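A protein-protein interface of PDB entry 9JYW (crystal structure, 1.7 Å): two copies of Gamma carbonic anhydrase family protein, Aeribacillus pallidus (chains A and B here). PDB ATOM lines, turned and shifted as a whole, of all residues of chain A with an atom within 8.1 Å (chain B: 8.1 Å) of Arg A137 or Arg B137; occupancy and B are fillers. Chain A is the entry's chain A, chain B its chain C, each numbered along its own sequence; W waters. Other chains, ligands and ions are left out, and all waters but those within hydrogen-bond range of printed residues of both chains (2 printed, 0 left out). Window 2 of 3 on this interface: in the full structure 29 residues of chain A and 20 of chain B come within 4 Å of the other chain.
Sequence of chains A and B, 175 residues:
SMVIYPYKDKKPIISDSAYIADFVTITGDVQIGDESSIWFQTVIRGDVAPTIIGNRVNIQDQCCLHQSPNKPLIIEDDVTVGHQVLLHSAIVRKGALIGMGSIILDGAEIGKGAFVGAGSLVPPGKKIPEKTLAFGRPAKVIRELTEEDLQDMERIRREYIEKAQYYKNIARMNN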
ATOM      1  N   MET A 100      23.162  -8.257  -7.567  1.00  0.00           N
ATOM      2  CA  MET A 100      24.432  -7.943  -6.890  1.00  0.00           C
ATOM      3  C   MET A 100      25.116  -9.244  -6.413  1.00  0.00           C
ATOM      4  O   MET A 100      24.434 -10.179  -5.955  1.00  0.00           O
ATOM      5  CB  MET A 100      24.173  -6.956  -5.751  1.00  0.00           C
ATOM      6  CG  MET A 100      23.304  -7.533  -4.651  1.00  0.00           C
ATOM      7  SD  MET A 100      22.892  -6.279  -3.411  1.00  0.00           S
ATOM      8  CE  MET A 100      21.407  -5.575  -4.113  1.00  0.00           C
ATOM      9  N   GLY A 101      26.440  -9.309  -6.586  1.00  0.00           N
ATOM     10  CA  GLY A 101      27.272 -10.416  -6.090  1.00  0.00           C
ATOM     11  C   GLY A 101      27.210 -11.652  -6.957  1.00  0.00           C
ATOM     12  O   GLY A 101      27.679 -12.711  -6.516  1.00  0.00           O
ATOM     13  N   SER A 102      26.637 -11.555  -8.161  1.00  0.00           N
ATOM     14  CA  SER A 102      26.528 -12.701  -9.090  1.00  0.00           C
ATOM     15  C   SER A 102      27.771 -12.809  -9.976  1.00  0.00           C
ATOM     16  O   SER A 102      28.489 -11.819 -10.166  1.00  0.00           O
ATOM     17  CB  SER A 102      25.262 -12.605  -9.942  1.00  0.00           C
ATOM     18  OG  SER A 102      24.115 -12.706  -9.124  1.00  0.00           O
ATOM     19  N   ILE A 103      27.931 -13.970 -10.568  1.00  0.00           N
ATOM     20  CA  ILE A 103      29.025 -14.308 -11.514  1.00  0.00           C
ATOM     21  C   ILE A 103      28.368 -14.904 -12.749  1.00  0.00           C
ATOM     22  O   ILE A 103      27.617 -15.891 -12.591  1.00  0.00           O
ATOM     23  CB  ILE A 103      30.045 -15.251 -10.855  1.00  0.00           C
ATOM     24  CG1 ILE A 103      31.095 -15.778 -11.821  1.00  0.00           C
ATOM     25  CG2 ILE A 103      29.351 -16.421 -10.158  1.00  0.00           C
ATOM     26  CD1 ILE A 103      32.064 -16.754 -11.163  1.00  0.00           C
ATOM     27  N   LEU A 105      29.165 -16.403 -16.447  1.00  0.00           N
ATOM     28  CA  LEU A 105      30.328 -16.891 -17.174  1.00  0.00           C
ATOM     29  C   LEU A 105      30.270 -17.032 -18.683  1.00  0.00           C
ATOM     30  O   LEU A 105      29.287 -16.701 -19.302  1.00  0.00           O
ATOM     31  CB  LEU A 105      30.782 -18.204 -16.506  1.00  0.00           C
ATOM     32  CG  LEU A 105      31.198 -18.031 -15.042  1.00  0.00           C
ATOM     33  CD1 LEU A 105      31.338 -19.346 -14.299  1.00  0.00           C
ATOM     34  CD2 LEU A 105      32.477 -17.216 -14.959  1.00  0.00           C
ATOM     35  N   GLY A 117      18.979 -13.539  -9.493  1.00  0.00           N
ATOM     36  CA  GLY A 117      18.946 -13.190  -8.064  1.00  0.00           C
ATOM     37  C   GLY A 117      20.355 -12.921  -7.544  1.00  0.00           C
ATOM     38  O   GLY A 117      21.325 -13.481  -8.072  1.00  0.00           O
ATOM     39  N   ALA A 118      20.455 -12.117  -6.473  1.00  0.00           N
ATOM     40  CA  ALA A 118      21.759 -11.808  -5.830  1.00  0.00           C
ATOM     41  C   ALA A 118      22.508 -13.120  -5.513  1.00  0.00           C
ATOM     42  O   ALA A 118      21.866 -14.137  -5.089  1.00  0.00           O
ATOM     43  CB  ALA A 118      21.528 -11.025  -4.573  1.00  0.00           C
ATOM     44  N   GLY A 119      23.825 -13.090  -5.699  1.00  0.00           N
ATOM     45  CA  GLY A 119      24.760 -14.123  -5.255  1.00  0.00           C
ATOM     46  C   GLY A 119      24.776 -15.331  -6.158  1.00  0.00           C
ATOM     47  O   GLY A 119      25.323 -16.365  -5.735  1.00  0.00           O
ATOM     48  N   SER A 120      24.193 -15.239  -7.354  1.00  0.00           N
ATOM     49  CA  SER A 120      24.036 -16.397  -8.251  1.00  0.00           C
ATOM     50  C   SER A 120      25.333 -16.663  -9.035  1.00  0.00           C
ATOM     51  O   SER A 120      26.163 -15.759  -9.197  1.00  0.00           O
ATOM     52  CB  SER A 120      22.877 -16.204  -9.211  1.00  0.00           C
ATOM     53  OG  SER A 120      21.648 -16.153  -8.523  1.00  0.00           O
ATOM     54  N   LEU A 121      25.427 -17.881  -9.574  1.00  0.00           N
ATOM     55  CA  LEU A 121      26.457 -18.270 -10.550  1.00  0.00           C
ATOM     56  C   LEU A 121      25.738 -18.834 -11.756  1.00  0.00           C
ATOM     57  O   LEU A 121      24.977 -19.814 -11.576  1.00  0.00           O
ATOM     58  CB  LEU A 121      27.451 -19.251  -9.922  1.00  0.00           C
ATOM     59  CG  LEU A 121      28.605 -19.678 -10.840  1.00  0.00           C
ATOM     60  CD1 LEU A 121      29.801 -20.108 -10.027  1.00  0.00           C
ATOM     61  CD2 LEU A 121      28.188 -20.793 -11.792  1.00  0.00           C
ATOM     62  N   VAL A 122      25.944 -18.229 -12.924  1.00  0.00           N
ATOM     63  CA  VAL A 122      25.428 -18.754 -14.214  1.00  0.00           C
ATOM     64  C   VAL A 122      26.610 -19.340 -14.976  1.00  0.00           C
ATOM     65  O   VAL A 122      27.508 -18.612 -15.397  1.00  0.00           O
ATOM     66  CB  VAL A 122      24.689 -17.694 -15.038  1.00  0.00           C
ATOM     67  CG1 VAL A 122      24.140 -18.310 -16.333  1.00  0.00           C
ATOM     68  CG2 VAL A 122      23.571 -17.078 -14.210  1.00  0.00           C
ATOM     69  N   PRO A 123      26.663 -20.687 -15.113  1.00  0.00           N
ATOM     70  CA  PRO A 123      27.812 -21.359 -15.692  1.00  0.00           C
ATOM     71  C   PRO A 123      27.961 -21.114 -17.194  1.00  0.00           C
ATOM     72  O   PRO A 123      27.038 -20.633 -17.860  1.00  0.00           O
ATOM     73  CB  PRO A 123      27.543 -22.864 -15.484  1.00  0.00           C
ATOM     74  CG  PRO A 123      26.383 -22.950 -14.581  1.00  0.00           C
ATOM     75  CD  PRO A 123      25.627 -21.634 -14.662  1.00  0.00           C
ATOM     76  N   ALA A 134      15.813 -16.322 -11.898  1.00  0.00           N
ATOM     77  CA  ALA A 134      16.716 -17.469 -11.704  1.00  0.00           C
ATOM     78  C   ALA A 134      17.706 -17.111 -10.590  1.00  0.00           C
ATOM     79  O   ALA A 134      18.181 -15.974 -10.584  1.00  0.00           O
ATOM     80  CB  ALA A 134      17.450 -17.761 -12.989  1.00  0.00           C
ATOM     81  N   PHE A 135      17.992 -18.033  -9.691  1.00  0.00           N
ATOM     82  CA  PHE A 135      19.030 -17.792  -8.662  1.00  0.00           C
ATOM     83  C   PHE A 135      19.605 -19.128  -8.221  1.00  0.00           C
ATOM     84  O   PHE A 135      19.037 -20.204  -8.516  1.00  0.00           O
ATOM     85  CB  PHE A 135      18.506 -16.916  -7.523  1.00  0.00           C
ATOM     86  CG  PHE A 135      17.452 -17.532  -6.640  1.00  0.00           C
ATOM     87  CD1 PHE A 135      17.746 -18.582  -5.782  1.00  0.00           C
ATOM     88  CD2 PHE A 135      16.167 -17.018  -6.629  1.00  0.00           C
ATOM     89  CE1 PHE A 135      16.769 -19.112  -4.946  1.00  0.00           C
ATOM     90  CE2 PHE A 135      15.187 -17.558  -5.801  1.00  0.00           C
ATOM     91  CZ  PHE A 135      15.493 -18.607  -4.966  1.00  0.00           C
ATOM     92  N   GLY A 136      20.743 -19.016  -7.537  1.00  0.00           N
ATOM     93  CA  GLY A 136      21.480 -20.156  -6.966  1.00  0.00           C
ATOM     94  C   GLY A 136      22.824 -20.335  -7.639  1.00  0.00           C
ATOM     95  O   GLY A 136      23.158 -19.528  -8.518  1.00  0.00           O
ATOM     96  N   ARG A 137      23.539 -21.384  -7.228  1.00  0.00           N
ATOM     97  CA  ARG A 137      24.892 -21.703  -7.735  1.00  0.00           C
ATOM     98  C   ARG A 137      24.974 -23.205  -7.971  1.00  0.00           C
ATOM     99  O   ARG A 137      25.190 -23.952  -7.012  1.00  0.00           O
ATOM    100  CB  ARG A 137      25.936 -21.279  -6.707  1.00  0.00           C
ATOM    101  CG  ARG A 137      25.891 -19.793  -6.393  1.00  0.00           C
ATOM    102  CD  ARG A 137      26.896 -19.478  -5.298  1.00  0.00           C
ATOM    103  NE  ARG A 137      28.263 -19.380  -5.808  1.00  0.00           N
ATOM    104  CZ  ARG A 137      28.847 -18.259  -6.243  1.00  0.00           C
ATOM    105  NH1 ARG A 137      28.185 -17.112  -6.269  1.00  0.00           N
ATOM    106  NH2 ARG A 137      30.110 -18.300  -6.628  1.00  0.00           N
ATOM    107  N   PRO A 138      24.766 -23.701  -9.213  1.00  0.00           N
ATOM    108  CA  PRO A 138      24.383 -22.876 -10.368  1.00  0.00           C
ATOM    109  C   PRO A 138      22.923 -22.418 -10.371  1.00  0.00           C
ATOM    110  O   PRO A 138      22.089 -23.080  -9.762  1.00  0.00           O
ATOM    111  CB  PRO A 138      24.619 -23.838 -11.547  1.00  0.00           C
ATOM    112  CG  PRO A 138      24.305 -25.201 -10.959  1.00  0.00           C
ATOM    113  CD  PRO A 138      24.887 -25.125  -9.562  1.00  0.00           C
ATOM    114  N   ALA A 139      22.633 -21.319 -11.081  1.00  0.00           N
ATOM    115  CA  ALA A 139      21.315 -20.662 -11.115  1.00  0.00           C
ATOM    116  C   ALA A 139      20.305 -21.625 -11.742  1.00  0.00           C
ATOM    117  O   ALA A 139      20.629 -22.262 -12.750  1.00  0.00           O
ATOM    118  CB  ALA A 139      21.379 -19.362 -11.879  1.00  0.00           C
ATOM    119  N   LYS A 140      19.134 -21.712 -11.114  1.00  0.00           N
ATOM    120  CA  LYS A 140      17.940 -22.454 -11.589  1.00  0.00           C
ATOM    121  C   LYS A 140      16.835 -21.443 -11.875  1.00  0.00           C
ATOM    122  O   LYS A 140      16.660 -20.518 -11.088  1.00  0.00           O
ATOM    123  CB  LYS A 140      17.482 -23.452 -10.528  1.00  0.00           C
ATOM    124  CG  LYS A 140      18.337 -24.698 -10.354  1.00  0.00           C
ATOM    125  CD  LYS A 140      17.640 -25.776  -9.525  1.00  0.00           C
ATOM    126  CE  LYS A 140      18.566 -26.568  -8.617  1.00  0.00           C
ATOM    127  NZ  LYS A 140      17.841 -27.169  -7.474  1.00  0.00           N
ATOM    128  N   MET B 100      38.184 -17.450 -11.275  1.00  0.00           N
ATOM    129  CA  MET B 100      37.591 -16.137 -10.938  1.00  0.00           C
ATOM    130  C   MET B 100      36.432 -16.293  -9.938  1.00  0.00           C
ATOM    131  O   MET B 100      35.647 -17.255 -10.038  1.00  0.00           O
ATOM    132  CB  MET B 100      37.176 -15.434 -12.234  1.00  0.00           C
ATOM    133  CG  MET B 100      36.055 -16.133 -12.971  1.00  0.00           C
ATOM    134  SD  MET B 100      35.777 -15.294 -14.574  1.00  0.00           S
ATOM    135  CE  MET B 100      36.854 -16.206 -15.657  1.00  0.00           C
ATOM    136  N   GLY B 101      36.370 -15.392  -8.972  1.00  0.00           N
ATOM    137  CA  GLY B 101      35.293 -15.303  -7.964  1.00  0.00           C
ATOM    138  C   GLY B 101      35.391 -16.361  -6.879  1.00  0.00           C
ATOM    139  O   GLY B 101      34.400 -16.552  -6.143  1.00  0.00           O
ATOM    140  N   SER B 102      36.540 -17.031  -6.758  1.00  0.00           N
ATOM    141  CA  SER B 102      36.772 -18.074  -5.729  1.00  0.00           C
ATOM    142  C   SER B 102      37.296 -17.428  -4.433  1.00  0.00           C
ATOM    143  O   SER B 102      37.827 -16.292  -4.451  1.00  0.00           O
ATOM    144  CB  SER B 102      37.714 -19.135  -6.200  1.00  0.00           C
ATOM    145  OG  SER B 102      37.146 -19.880  -7.266  1.00  0.00           O
ATOM    146  N   ILE B 103      37.134 -18.163  -3.340  1.00  0.00           N
ATOM    147  CA  ILE B 103      37.691 -17.800  -2.017  1.00  0.00           C
ATOM    148  C   ILE B 103      38.492 -18.974  -1.500  1.00  0.00           C
ATOM    149  O   ILE B 103      37.956 -20.082  -1.435  1.00  0.00           O
ATOM    150  CB  ILE B 103      36.573 -17.361  -1.060  1.00  0.00           C
ATOM    151  CG1 ILE B 103      35.548 -18.430  -0.764  1.00  0.00           C
ATOM    152  CG2 ILE B 103      35.851 -16.179  -1.651  1.00  0.00           C
ATOM    153  CD1 ILE B 103      34.605 -17.933   0.330  1.00  0.00           C
ATOM    154  N   LEU B 105      40.784 -20.134   1.723  1.00  0.00           N
ATOM    155  CA  LEU B 105      40.872 -19.688   3.134  1.00  0.00           C
ATOM    156  C   LEU B 105      42.077 -20.312   3.856  1.00  0.00           C
ATOM    157  O   LEU B 105      42.922 -20.958   3.210  1.00  0.00           O
ATOM    158  CB  LEU B 105      39.547 -20.018   3.811  1.00  0.00           C
ATOM    159  CG  LEU B 105      38.374 -19.212   3.255  1.00  0.00           C
ATOM    160  CD1 LEU B 105      37.056 -19.732   3.769  1.00  0.00           C
ATOM    161  CD2 LEU B 105      38.546 -17.733   3.549  1.00  0.00           C
ATOM    162  N   GLY B 117      37.680 -24.379  -9.955  1.00  0.00           N
ATOM    163  CA  GLY B 117      36.654 -23.790 -10.833  1.00  0.00           C
ATOM    164  C   GLY B 117      36.179 -22.448 -10.322  1.00  0.00           C
ATOM    165  O   GLY B 117      36.225 -22.209  -9.092  1.00  0.00           O
ATOM    166  N   ALA B 118      35.686 -21.595 -11.224  1.00  0.00           N
ATOM    167  CA  ALA B 118      35.111 -20.274 -10.877  1.00  0.00           C
ATOM    168  C   ALA B 118      34.084 -20.421  -9.750  1.00  0.00           C
ATOM    169  O   ALA B 118      33.278 -21.406  -9.769  1.00  0.00           O
ATOM    170  CB  ALA B 118      34.508 -19.616 -12.086  1.00  0.00           C
ATOM    171  N   GLY B 119      34.099 -19.474  -8.813  1.00  0.00           N
ATOM    172  CA  GLY B 119      33.048 -19.289  -7.803  1.00  0.00           C
ATOM    173  C   GLY B 119      33.183 -20.268  -6.659  1.00  0.00           C
ATOM    174  O   GLY B 119      32.244 -20.398  -5.891  1.00  0.00           O
ATOM    175  N   SER B 120      34.333 -20.946  -6.522  1.00  0.00           N
ATOM    176  CA  SER B 120      34.520 -22.009  -5.505  1.00  0.00           C
ATOM    177  C   SER B 120      34.884 -21.405  -4.148  1.00  0.00           C
ATOM    178  O   SER B 120      35.366 -20.259  -4.072  1.00  0.00           O
ATOM    179  CB  SER B 120      35.553 -23.000  -5.937  1.00  0.00           C
ATOM    180  OG  SER B 120      35.140 -23.712  -7.101  1.00  0.00           O
ATOM    181  N   LEU B 121      34.697 -22.198  -3.098  1.00  0.00           N
ATOM    182  CA  LEU B 121      35.187 -21.899  -1.734  1.00  0.00           C
ATOM    183  C   LEU B 121      36.006 -23.101  -1.283  1.00  0.00           C
ATOM    184  O   LEU B 121      35.436 -24.226  -1.278  1.00  0.00           O
ATOM    185  CB  LEU B 121      34.019 -21.606  -0.784  1.00  0.00           C
ATOM    186  CG  LEU B 121      34.439 -21.202   0.628  1.00  0.00           C
ATOM    187  CD1 LEU B 121      33.396 -20.312   1.282  1.00  0.00           C
ATOM    188  CD2 LEU B 121      34.686 -22.426   1.484  1.00  0.00           C
ATOM    189  N   VAL B 122      37.275 -22.884  -0.978  1.00  0.00           N
ATOM    190  CA  VAL B 122      38.150 -23.916  -0.349  1.00  0.00           C
ATOM    191  C   VAL B 122      38.334 -23.564   1.122  1.00  0.00           C
ATOM    192  O   VAL B 122      38.954 -22.553   1.453  1.00  0.00           O
ATOM    193  CB  VAL B 122      39.496 -24.075  -1.066  1.00  0.00           C
ATOM    194  CG1 VAL B 122      40.327 -25.176  -0.414  1.00  0.00           C
ATOM    195  CG2 VAL B 122      39.272 -24.361  -2.539  1.00  0.00           C
ATOM    196  N   PRO B 123      37.722 -24.349   2.034  1.00  0.00           N
ATOM    197  CA  PRO B 123      37.706 -24.014   3.460  1.00  0.00           C
ATOM    198  C   PRO B 123      39.075 -24.125   4.128  1.00  0.00           C
ATOM    199  O   PRO B 123      40.011 -24.706   3.571  1.00  0.00           O
ATOM    200  CB  PRO B 123      36.753 -25.031   4.105  1.00  0.00           C
ATOM    201  CG  PRO B 123      36.135 -25.797   2.986  1.00  0.00           C
ATOM    202  CD  PRO B 123      36.991 -25.588   1.747  1.00  0.00           C
ATOM    203  N   ALA B 134      38.694 -29.110  -9.143  1.00  0.00           N
ATOM    204  CA  ALA B 134      37.819 -29.048  -7.953  1.00  0.00           C
ATOM    205  C   ALA B 134      36.942 -27.806  -8.099  1.00  0.00           C
ATOM    206  O   ALA B 134      37.450 -26.769  -8.531  1.00  0.00           O
ATOM    207  CB  ALA B 134      38.619 -28.981  -6.685  1.00  0.00           C
ATOM    208  N   PHE B 135      35.668 -27.904  -7.760  1.00  0.00           N
ATOM    209  CA  PHE B 135      34.786 -26.721  -7.722  1.00  0.00           C
ATOM    210  C   PHE B 135      33.642 -26.992  -6.751  1.00  0.00           C
ATOM    211  O   PHE B 135      33.407 -28.143  -6.342  1.00  0.00           O
ATOM    212  CB  PHE B 135      34.343 -26.305  -9.131  1.00  0.00           C
ATOM    213  CG  PHE B 135      33.429 -27.261  -9.853  1.00  0.00           C
ATOM    214  CD1 PHE B 135      32.117 -27.434  -9.448  1.00  0.00           C
ATOM    215  CD2 PHE B 135      33.874 -27.969 -10.968  1.00  0.00           C
ATOM    216  CE1 PHE B 135      31.271 -28.301 -10.131  1.00  0.00           C
ATOM    217  CE2 PHE B 135      33.025 -28.825 -11.653  1.00  0.00           C
ATOM    218  CZ  PHE B 135      31.730 -29.003 -11.221  1.00  0.00           C
ATOM    219  N   GLY B 136      32.983 -25.910  -6.388  1.00  0.00           N
ATOM    220  CA  GLY B 136      31.820 -25.878  -5.485  1.00  0.00           C
ATOM    221  C   GLY B 136      32.134 -25.168  -4.189  1.00  0.00           C
ATOM    222  O   GLY B 136      33.262 -24.647  -4.042  1.00  0.00           O
ATOM    223  N   ARG B 137      31.165 -25.166  -3.283  1.00  0.00           N
ATOM    224  CA  ARG B 137      31.247 -24.454  -1.987  1.00  0.00           C
ATOM    225  C   ARG B 137      30.671 -25.350  -0.907  1.00  0.00           C
ATOM    226  O   ARG B 137      29.446 -25.419  -0.798  1.00  0.00           O
ATOM    227  CB  ARG B 137      30.470 -23.143  -2.047  1.00  0.00           C
ATOM    228  CG  ARG B 137      30.967 -22.194  -3.125  1.00  0.00           C
ATOM    229  CD  ARG B 137      30.095 -20.965  -3.156  1.00  0.00           C
ATOM    230  NE  ARG B 137      30.390 -19.989  -2.113  1.00  0.00           N
ATOM    231  CZ  ARG B 137      31.246 -18.973  -2.251  1.00  0.00           C
ATOM    232  NH1 ARG B 137      31.918 -18.803  -3.375  1.00  0.00           N
ATOM    233  NH2 ARG B 137      31.413 -18.107  -1.267  1.00  0.00           N
ATOM    234  N   PRO B 138      31.501 -26.108  -0.150  1.00  0.00           N
ATOM    235  CA  PRO B 138      32.942 -26.224  -0.362  1.00  0.00           C
ATOM    236  C   PRO B 138      33.359 -27.051  -1.587  1.00  0.00           C
ATOM    237  O   PRO B 138      32.590 -27.914  -2.012  1.00  0.00           O
ATOM    238  CB  PRO B 138      33.397 -26.951   0.906  1.00  0.00           C
ATOM    239  CG  PRO B 138      32.227 -27.864   1.248  1.00  0.00           C
ATOM    240  CD  PRO B 138      31.022 -26.997   0.933  1.00  0.00           C
ATOM    241  N   ALA B 139      34.562 -26.795  -2.115  1.00  0.00           N
ATOM    242  CA  ALA B 139      35.078 -27.407  -3.355  1.00  0.00           C
ATOM    243  C   ALA B 139      35.205 -28.925  -3.148  1.00  0.00           C
ATOM    244  O   ALA B 139      35.686 -29.345  -2.076  1.00  0.00           O
ATOM    245  CB  ALA B 139      36.392 -26.782  -3.750  1.00  0.00           C
ATOM    246  N   LYS B 140      34.766 -29.675  -4.155  1.00  0.00           N
ATOM    247  CA  LYS B 140      34.922 -31.141  -4.267  1.00  0.00           C
ATOM    248  C   LYS B 140      35.841 -31.431  -5.450  1.00  0.00           C
ATOM    249  O   LYS B 140      35.706 -30.797  -6.520  1.00  0.00           O
ATOM    250  CB  LYS B 140      33.562 -31.803  -4.490  1.00  0.00           C
ATOM    251  CG  LYS B 140      32.637 -31.870  -3.283  1.00  0.00           C
ATOM    252  CD  LYS B 140      31.217 -32.225  -3.688  1.00  0.00           C
ATOM    253  CE  LYS B 140      30.445 -33.001  -2.643  1.00  0.00           C
ATOM    254  NZ  LYS B 140      29.028 -33.153  -3.048  1.00  0.00           N
HETATM  255  O   HOH W   1      31.930 -16.097  -7.359  1.00  0.00           O
HETATM  256  O   HOH W   2      29.558 -22.201  -6.461  1.00  0.00           O
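Met B100 touches Ile A103. Ile A103 touches Ala B118. Leu A105 touches Met B100 (CD2 to SD, 3.8 Å). CD1 of Leu A105 touches CB of Ala B118, at 3.9 Å. Ala B118 touches Leu A121. Arg A137 touches Arg B137.
Water W1 bridges the backbone carbonyl oxygen (O) of Gly B101 (2.8 Å) and the guanidinium group (NH2) of Arg A137 (2.9 Å). Water W2 lies within hydrogen-bond range of NE of Arg A137 (3.2 Å) and O of Gly B119 (3.3 Å).
Hydrophobic or aromatic side chains of chain B within 4 Å of the printed part of chain A: Met B100 and Ala B118. Hydrophobic or aromatic side chains of chain A within 4 Å of the printed part of chain B: Ile A103, Leu A105 and Leu A121. Among the printed residues, 7 pairs touch across the chains. Among the printed residues, no Asp or Glu carboxylate lies within 4 Å of a Lys or Arg side-chain nitrogen of the other chain.
O of Gly B119 lies within hydrogen-bond range of NH2 of Arg A137 (3.1 Å).
Printed residues of chain B within 4 Å of Arg A137: Gly B119 (3.1 Å) and Arg B137 (3.6 Å). Printed residues of chain A within 4 Å of Arg B137: Arg A137. No residue of chain B comes within 4 Å of Gly A136. No residue of chain B comes within 4 Å of Pro A138. No residue of chain A comes within 4 Å of Gly B136. Pro B138 touches none of the printed residues of chain A. Printed residues of chain A within 4 Å of Gly B119: Arg A137. Printed residues of chain B within 4 Å of Leu A105: Met B100 and Ala B118. Of the printed residues of chain A, Ala B118 touches Ile A103 (3.9 Å), Leu A105 (3.9 Å) and Leu A121 (3.7 Å). The nearest residue of chain A that does not touch Arg B137 is Leu A121 (6.9 Å). The nearest printed residue of chain A that does not touch Ala B118 is Arg A137 (5.4 Å).
Ile A103 touches Ala B118, but with the chains exchanged Ala A118 does not touch Ile B103 (14.2 Å). Leu A105 touches Met B100, but with the chains exchanged Met A100 does not touch Leu B105 (18.6 Å). Leu A105 touches Ala B118, but with the chains exchanged Ala A118 does not touch Leu B105 (18.5 Å). Leu A121 touches Ala B118, but with the chains exchanged Ala A118 does not touch Leu B121 (14.5 Å). Of the 7 pairs that touch across the chains among the printed residues, 1 has its exchanged pair printed and touching as well.
N of Ile A103 sits at hydrogen-bond distance from O of Ser A120. The guanidinium group of Arg A137 sits at hydrogen-bond distance from the backbone carbonyl oxygen of Gly A119, 3.0 Å away. The backbone NH of Leu A121 is in hydrogen-bond range of the backbone carbonyl oxygen of Gly A136 (3.0 Å). N of Gly B119 is in hydrogen-bond range of O of Met B100, at 3.0 Å. The backbone NH (N) of Gly B119 sits at hydrogen-bond distance from the side-chain hydroxyl (OG) of Ser B102, 3.4 Å away. The backbone carbonyl oxygen of Gly B119 lies within hydrogen-bond range of the guanidinium group of Arg B137 (3.0 Å).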
